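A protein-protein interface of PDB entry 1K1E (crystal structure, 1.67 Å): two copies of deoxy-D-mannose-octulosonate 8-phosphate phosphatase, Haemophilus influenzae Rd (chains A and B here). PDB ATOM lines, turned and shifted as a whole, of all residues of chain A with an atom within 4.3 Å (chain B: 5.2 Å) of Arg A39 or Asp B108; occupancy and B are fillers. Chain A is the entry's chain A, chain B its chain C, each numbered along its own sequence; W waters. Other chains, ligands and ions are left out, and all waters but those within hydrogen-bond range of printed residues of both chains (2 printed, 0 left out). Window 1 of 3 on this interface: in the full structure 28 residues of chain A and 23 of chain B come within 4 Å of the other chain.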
ATOM      1  N   HIS A  37      27.009  -0.226  24.257  1.00  0.00           N
ATOM      2  CA  HIS A  37      27.337   0.886  25.142  1.00  0.00           C
ATOM      3  C   HIS A  37      26.056   1.429  25.716  1.00  0.00           C
ATOM      4  O   HIS A  37      25.084   1.686  24.975  1.00  0.00           O
ATOM      5  CB  HIS A  37      28.128   1.956  24.376  1.00  0.00           C
ATOM      6  CG  HIS A  37      28.648   3.032  25.259  1.00  0.00           C
ATOM      7  ND1 HIS A  37      29.988   3.178  25.564  1.00  0.00           N
ATOM      8  CD2 HIS A  37      27.989   3.996  25.957  1.00  0.00           C
ATOM      9  CE1 HIS A  37      30.136   4.197  26.409  1.00  0.00           C
ATOM     10  NE2 HIS A  37      28.942   4.706  26.656  1.00  0.00           N
ATOM     11  N   VAL A  38      26.060   1.626  27.027  1.00  0.00           N
ATOM     12  CA  VAL A  38      24.832   2.063  27.692  1.00  0.00           C
ATOM     13  C   VAL A  38      24.295   3.411  27.186  1.00  0.00           C
ATOM     14  O   VAL A  38      23.081   3.566  27.094  1.00  0.00           O
ATOM     15  CB  VAL A  38      25.066   2.128  29.193  1.00  0.00           C
ATOM     16  CG1 VAL A  38      26.042   3.294  29.525  1.00  0.00           C
ATOM     17  CG2 VAL A  38      23.743   2.216  29.934  1.00  0.00           C
ATOM     18  N   ARG A  39      25.177   4.382  26.887  1.00  0.00           N
ATOM     19  CA  ARG A  39      24.629   5.665  26.461  1.00  0.00           C
ATOM     20  C   ARG A  39      24.039   5.600  25.019  1.00  0.00           C
ATOM     21  O   ARG A  39      23.152   6.397  24.662  1.00  0.00           O
ATOM     22  CB  ARG A  39      25.642   6.769  26.599  1.00  0.00           C
ATOM     23  CG  ARG A  39      26.232   6.849  28.065  1.00  0.00           C
ATOM     24  CD  ARG A  39      26.956   8.186  28.394  1.00  0.00           C
ATOM     25  NE  ARG A  39      28.263   8.229  27.728  1.00  0.00           N
ATOM     26  CZ  ARG A  39      29.374   7.695  28.252  1.00  0.00           C
ATOM     27  NH1 ARG A  39      29.394   7.066  29.432  1.00  0.00           N
ATOM     28  NH2 ARG A  39      30.493   7.812  27.587  1.00  0.00           N
ATOM     29  N   ASP A  40      24.540   4.683  24.180  1.00  0.00           N
ATOM     30  CA  ASP A  40      23.890   4.482  22.888  1.00  0.00           C
ATOM     31  C   ASP A  40      22.411   3.978  23.115  1.00  0.00           C
ATOM     32  O   ASP A  40      21.462   4.372  22.412  1.00  0.00           O
ATOM     33  CB  ASP A  40      24.591   3.386  22.093  1.00  0.00           C
ATOM     34  CG  ASP A  40      25.948   3.852  21.482  1.00  0.00           C
ATOM     35  OD1 ASP A  40      26.122   5.061  21.306  1.00  0.00           O
ATOM     36  OD2 ASP A  40      26.805   3.019  21.126  1.00  0.00           O
ATOM     37  N   GLY A  41      22.278   3.032  24.025  1.00  0.00           N
ATOM     38  CA  GLY A  41      20.971   2.483  24.283  1.00  0.00           C
ATOM     39  C   GLY A  41      20.049   3.586  24.747  1.00  0.00           C
ATOM     40  O   GLY A  41      18.893   3.593  24.372  1.00  0.00           O
ATOM     41  N   LEU A  42      20.512   4.512  25.565  1.00  0.00           N
ATOM     42  CA  LEU A  42      19.616   5.587  25.947  1.00  0.00           C
ATOM     43  C   LEU A  42      19.305   6.514  24.747  1.00  0.00           C
ATOM     44  O   LEU A  42      18.194   7.018  24.614  1.00  0.00           O
ATOM     45  CB  LEU A  42      20.218   6.410  27.085  1.00  0.00           C
ATOM     46  CG  LEU A  42      19.353   7.559  27.572  1.00  0.00           C
ATOM     47  CD1 LEU A  42      18.027   6.947  28.041  1.00  0.00           C
ATOM     48  CD2 LEU A  42      20.016   8.321  28.679  1.00  0.00           C
ATOM     49  N   GLY A  43      20.289   6.724  23.874  1.00  0.00           N
ATOM     50  CA  GLY A  43      20.059   7.552  22.702  1.00  0.00           C
ATOM     51  C   GLY A  43      18.981   6.906  21.820  1.00  0.00           C
ATOM     52  O   GLY A  43      18.149   7.615  21.186  1.00  0.00           O
ATOM     53  N   ARG A 149      25.129   7.593  20.217  1.00  0.00           N
ATOM     54  CA  ARG A 149      24.582   8.653  21.084  1.00  0.00           C
ATOM     55  C   ARG A 149      25.003  10.045  20.607  1.00  0.00           C
ATOM     56  O   ARG A 149      24.228  10.981  20.662  1.00  0.00           O
ATOM     57  CB  ARG A 149      25.072   8.446  22.510  1.00  0.00           C
ATOM     58  CG  ARG A 149      24.486   9.435  23.502  1.00  0.00           C
ATOM     59  CD  ARG A 149      22.979   9.539  23.489  1.00  0.00           C
ATOM     60  NE  ARG A 149      22.539  10.512  24.513  1.00  0.00           N
ATOM     61  CZ  ARG A 149      22.431  10.223  25.793  1.00  0.00           C
ATOM     62  NH1 ARG A 149      22.711   8.998  26.235  1.00  0.00           N
ATOM     63  NH2 ARG A 149      22.064  11.165  26.630  1.00  0.00           N
ATOM     64  N   GLY B  17      28.863   3.338  33.064  1.00  0.00           N
ATOM     65  CA  GLY B  17      29.535   4.548  32.631  1.00  0.00           C
ATOM     66  C   GLY B  17      30.289   5.238  33.781  1.00  0.00           C
ATOM     67  O   GLY B  17      30.968   6.227  33.515  1.00  0.00           O
ATOM     68  N   ASP B  21      33.018   1.332  32.144  1.00  0.00           N
ATOM     69  CA  ASP B  21      33.330   2.258  31.057  1.00  0.00           C
ATOM     70  C   ASP B  21      32.143   2.426  30.140  1.00  0.00           C
ATOM     71  O   ASP B  21      32.278   2.910  29.015  1.00  0.00           O
ATOM     72  CB  ASP B  21      34.556   1.784  30.283  1.00  0.00           C
ATOM     73  CG  ASP B  21      34.334   0.518  29.556  1.00  0.00           C
ATOM     74  OD1 ASP B  21      33.245  -0.058  29.711  1.00  0.00           O
ATOM     75  OD2 ASP B  21      35.266   0.085  28.822  1.00  0.00           O
ATOM     76  N   GLY B  22      30.994   1.900  30.600  1.00  0.00           N
ATOM     77  CA  GLY B  22      29.736   2.044  29.879  1.00  0.00           C
ATOM     78  C   GLY B  22      29.362   0.882  28.960  1.00  0.00           C
ATOM     79  O   GLY B  22      28.257   0.894  28.404  1.00  0.00           O
ATOM     80  N   GLY B 106      27.898  10.799  38.338  1.00  0.00           N
ATOM     81  CA  GLY B 106      27.152  10.221  37.217  1.00  0.00           C
ATOM     82  C   GLY B 106      27.819  10.399  35.869  1.00  0.00           C
ATOM     83  O   GLY B 106      28.862  11.038  35.792  1.00  0.00           O
ATOM     84  N   ASP B 107      27.191   9.879  34.808  1.00  0.00           N
ATOM     85  CA  ASP B 107      27.721  10.061  33.441  1.00  0.00           C
ATOM     86  C   ASP B 107      26.736  10.438  32.390  1.00  0.00           C
ATOM     87  O   ASP B 107      27.142  10.786  31.280  1.00  0.00           O
ATOM     88  CB  ASP B 107      28.405   8.770  32.902  1.00  0.00           C
ATOM     89  CG  ASP B 107      27.392   7.637  32.654  1.00  0.00           C
ATOM     90  OD1 ASP B 107      27.467   6.935  31.640  1.00  0.00           O
ATOM     91  OD2 ASP B 107      26.551   7.468  33.486  1.00  0.00           O
ATOM     92  N   ASP B 108      25.448  10.401  32.682  1.00  0.00           N
ATOM     93  CA  ASP B 108      24.502  10.618  31.624  1.00  0.00           C
ATOM     94  C   ASP B 108      23.217  11.354  31.980  1.00  0.00           C
ATOM     95  O   ASP B 108      23.009  11.773  33.113  1.00  0.00           O
ATOM     96  CB  ASP B 108      24.201   9.236  30.987  1.00  0.00           C
ATOM     97  CG  ASP B 108      23.725   9.369  29.559  1.00  0.00           C
ATOM     98  OD1 ASP B 108      23.399   8.335  28.920  1.00  0.00           O
ATOM     99  OD2 ASP B 108      23.688  10.517  29.077  1.00  0.00           O
ATOM    100  N   SER B 109      22.350  11.560  31.003  1.00  0.00           N
ATOM    101  CA  SER B 109      21.160  12.342  31.296  1.00  0.00           C
ATOM    102  C   SER B 109      20.287  11.800  32.440  1.00  0.00           C
ATOM    103  O   SER B 109      19.670  12.570  33.175  1.00  0.00           O
ATOM    104  CB  SER B 109      20.324  12.490  30.028  1.00  0.00           C
ATOM    105  OG  SER B 109      21.110  12.984  28.948  1.00  0.00           O
ATOM    106  N   VAL B 110      20.250  10.483  32.580  1.00  0.00           N
ATOM    107  CA  VAL B 110      19.506   9.871  33.638  1.00  0.00           C
ATOM    108  C   VAL B 110      19.944  10.409  34.964  1.00  0.00           C
ATOM    109  O   VAL B 110      19.133  10.412  35.915  1.00  0.00           O
ATOM    110  CB  VAL B 110      19.712   8.353  33.721  1.00  0.00           C
ATOM    111  CG1 VAL B 110      18.632   7.692  34.634  1.00  0.00           C
ATOM    112  CG2 VAL B 110      19.737   7.739  32.328  1.00  0.00           C
ATOM    113  N   ASP B 111      21.223  10.837  35.052  1.00  0.00           N
ATOM    114  CA  ASP B 111      21.736  11.361  36.296  1.00  0.00           C
ATOM    115  C   ASP B 111      21.443  12.822  36.595  1.00  0.00           C
ATOM    116  O   ASP B 111      21.669  13.260  37.756  1.00  0.00           O
ATOM    117  CB  ASP B 111      23.220  11.104  36.362  1.00  0.00           C
ATOM    118  CG  ASP B 111      23.521   9.637  36.120  1.00  0.00           C
ATOM    119  OD1 ASP B 111      22.983   8.828  36.908  1.00  0.00           O
ATOM    120  OD2 ASP B 111      24.223   9.312  35.136  1.00  0.00           O
ATOM    121  N   LEU B 112      20.897  13.558  35.618  1.00  0.00           N
ATOM    122  CA  LEU B 112      20.618  14.970  35.864  1.00  0.00           C
ATOM    123  C   LEU B 112      19.762  15.231  37.104  1.00  0.00           C
ATOM    124  O   LEU B 112      20.031  16.144  37.840  1.00  0.00           O
ATOM    125  CB  LEU B 112      19.994  15.632  34.645  1.00  0.00           C
ATOM    126  CG  LEU B 112      21.059  15.666  33.510  1.00  0.00           C
ATOM    127  CD1 LEU B 112      20.366  16.128  32.213  1.00  0.00           C
ATOM    128  CD2 LEU B 112      22.140  16.642  33.888  1.00  0.00           C
ATOM    129  N   PHE B 115      21.898  14.737  40.200  1.00  0.00           N
ATOM    130  CA  PHE B 115      22.802  15.854  40.515  1.00  0.00           C
ATOM    131  C   PHE B 115      22.018  16.977  41.232  1.00  0.00           C
ATOM    132  O   PHE B 115      22.501  17.600  42.174  1.00  0.00           O
ATOM    133  CB  PHE B 115      23.378  16.442  39.251  1.00  0.00           C
ATOM    134  CG  PHE B 115      24.129  15.462  38.382  1.00  0.00           C
ATOM    135  CD1 PHE B 115      24.084  15.624  37.001  1.00  0.00           C
ATOM    136  CD2 PHE B 115      24.952  14.480  38.926  1.00  0.00           C
ATOM    137  CE1 PHE B 115      24.855  14.822  36.142  1.00  0.00           C
ATOM    138  CE2 PHE B 115      25.738  13.651  38.102  1.00  0.00           C
ATOM    139  CZ  PHE B 115      25.708  13.803  36.711  1.00  0.00           C
ATOM    140  N   ASP B 126      34.409  11.336  30.517  1.00  0.00           N
ATOM    141  CA  ASP B 126      33.793  11.073  29.230  1.00  0.00           C
ATOM    142  C   ASP B 126      32.283  11.304  29.193  1.00  0.00           C
ATOM    143  O   ASP B 126      31.597  10.900  28.253  1.00  0.00           O
ATOM    144  CB  ASP B 126      34.161   9.671  28.700  1.00  0.00           C
ATOM    145  CG  ASP B 126      33.806   8.521  29.658  1.00  0.00           C
ATOM    146  OD1 ASP B 126      33.668   7.417  29.085  1.00  0.00           O
ATOM    147  OD2 ASP B 126      33.715   8.693  30.929  1.00  0.00           O
ATOM    148  N   ALA B 127      31.772  11.969  30.231  1.00  0.00           N
ATOM    149  CA  ALA B 127      30.380  12.348  30.243  1.00  0.00           C
ATOM    150  C   ALA B 127      30.145  13.401  29.156  1.00  0.00           C
ATOM    151  O   ALA B 127      31.025  14.218  28.807  1.00  0.00           O
ATOM    152  CB  ALA B 127      30.001  12.929  31.643  1.00  0.00           C
ATOM    153  N   PRO B 128      28.919  13.459  28.630  1.00  0.00           N
ATOM    154  CA  PRO B 128      28.677  14.472  27.601  1.00  0.00           C
ATOM    155  C   PRO B 128      28.642  15.874  28.143  1.00  0.00           C
ATOM    156  O   PRO B 128      28.395  16.106  29.320  1.00  0.00           O
ATOM    157  CB  PRO B 128      27.319  14.085  27.000  1.00  0.00           C
ATOM    158  CG  PRO B 128      26.618  13.420  28.166  1.00  0.00           C
ATOM    159  CD  PRO B 128      27.692  12.719  28.984  1.00  0.00           C
ATOM    160  N   TYR B 130      26.482  18.326  28.185  1.00  0.00           N
ATOM    161  CA  TYR B 130      25.335  18.750  29.012  1.00  0.00           C
ATOM    162  C   TYR B 130      25.347  18.105  30.412  1.00  0.00           C
ATOM    163  O   TYR B 130      24.691  18.614  31.335  1.00  0.00           O
ATOM    164  CB  TYR B 130      24.004  18.475  28.272  1.00  0.00           C
ATOM    165  CG  TYR B 130      23.999  17.112  27.599  1.00  0.00           C
ATOM    166  CD1 TYR B 130      23.540  15.973  28.269  1.00  0.00           C
ATOM    167  CD2 TYR B 130      24.451  16.976  26.305  1.00  0.00           C
ATOM    168  CE1 TYR B 130      23.518  14.733  27.650  1.00  0.00           C
ATOM    169  CE2 TYR B 130      24.439  15.700  25.646  1.00  0.00           C
ATOM    170  CZ  TYR B 130      23.967  14.599  26.318  1.00  0.00           C
ATOM    171  OH  TYR B 130      23.881  13.411  25.647  1.00  0.00           O
ATOM    172  N   VAL B 131      26.050  16.994  30.603  1.00  0.00           N
ATOM    173  CA  VAL B 131      26.141  16.420  31.949  1.00  0.00           C
ATOM    174  C   VAL B 131      27.313  17.133  32.654  1.00  0.00           C
ATOM    175  O   VAL B 131      27.181  17.576  33.764  1.00  0.00           O
ATOM    176  CB  VAL B 131      26.372  14.867  31.913  1.00  0.00           C
ATOM    177  CG1 VAL B 131      26.966  14.356  33.259  1.00  0.00           C
ATOM    178  CG2 VAL B 131      25.074  14.195  31.623  1.00  0.00           C
HETATM  179  O   HOH W   1      25.223  10.942  26.740  1.00  0.00           O
HETATM  180  O   HOH W   2      31.676   6.175  30.749  1.00  0.00           O
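The backbone carbonyl oxygen of Gly B22 sits at hydrogen-bond distance from the backbone NH of Val A38, 2.7 Å away. The guanidinium group of Arg A39 is in salt-bridge range of the side-chain carboxylate of Asp B107 (2.9 Å). The guanidinium group (NH2) of Arg A39 lies within salt-bridge range of the side-chain carboxylate (OD1) of Asp B126, at 3.5 Å. OD1 of Asp B108 is in salt-bridge range of NH1 of Arg A149 (2.8 Å). The guanidinium group of Arg A149 sits at hydrogen-bond distance from the side-chain hydroxyl of Ser B109, at 3.1 Å. NH2 of Arg A149 is in hydrogen-bond range of OH of Tyr B130, at 3.1 Å.
The guanidinium group (NH1) of Arg A149 lies within hydrogen-bond range of the backbone carbonyl oxygen (O) of Arg A39, 3.1 Å away. OD1 of Asp A40 sits at hydrogen-bond distance from N of Arg A149 (2.9 Å). N of Asp B107 sits at hydrogen-bond distance from OD2 of Asp B111. The backbone NH (N) of Asp B108 sits at hydrogen-bond distance from the side-chain carboxylate (OD2) of Asp B111 (3.0 Å).
Among the printed residues, pairs that only touch across the chains: Arg A39 with Asp B108 (3.3 Å), His A37 with Gly B22 (3.4 Å), Leu A42 with Asp B108 (3.4 Å), His A37 with Asp B21 (3.6 Å) and Leu A42 with Val B110 (3.7 Å).
Of the printed residues of chain B, His A37 touches Asp B21 and Gly B22. Printed residues of chain B within 4 Å of Arg A149: Asp B108 (2.8 Å), Ser B109 (3.1 Å) and Tyr B130 (3.1 Å). Printed residues of chain A within 4 Å of Asp B107: Arg A39 (2.9 Å). Printed residues of chain A within 4 Å of Asp B108: Arg A39 (3.3 Å), Leu A42 (3.4 Å) and Arg A149 (2.8 Å). Of the printed residues of chain A, Ser B109 touches Arg A149. Printed residues of chain A within 4 Å of Asp B126: Arg A39 (3.3 Å). The nearest residue of chain B that does not touch Arg A39 is Gly B17 (4.1 Å). The nearest printed residue of chain A that does not touch Asp B108 is Val A38 (5.1 Å).
Of the 8 printed residues of chain A, 5 touch a printed residue of chain B. Among the printed residues, 11 pairs touch across the chains.
No position is printed for both chains. Of the 11 pairs that touch across the chains among the printed residues, none has its exchanged pair printed and touching as well.
Water W2 lies within hydrogen-bond range of NH1 of Arg A39 (2.8 Å), O of Gly B17 (2.9 Å) and OD1 of Asp B126 (2.9 Å). Water W1 lies within hydrogen-bond range of the side-chain carboxylate (OD2) of Asp B108 (2.8 Å), the side-chain hydroxyl (OH) of Tyr B130 (3.0 Å) and the guanidinium group (NH2) of Arg A149 (3.2 Å).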
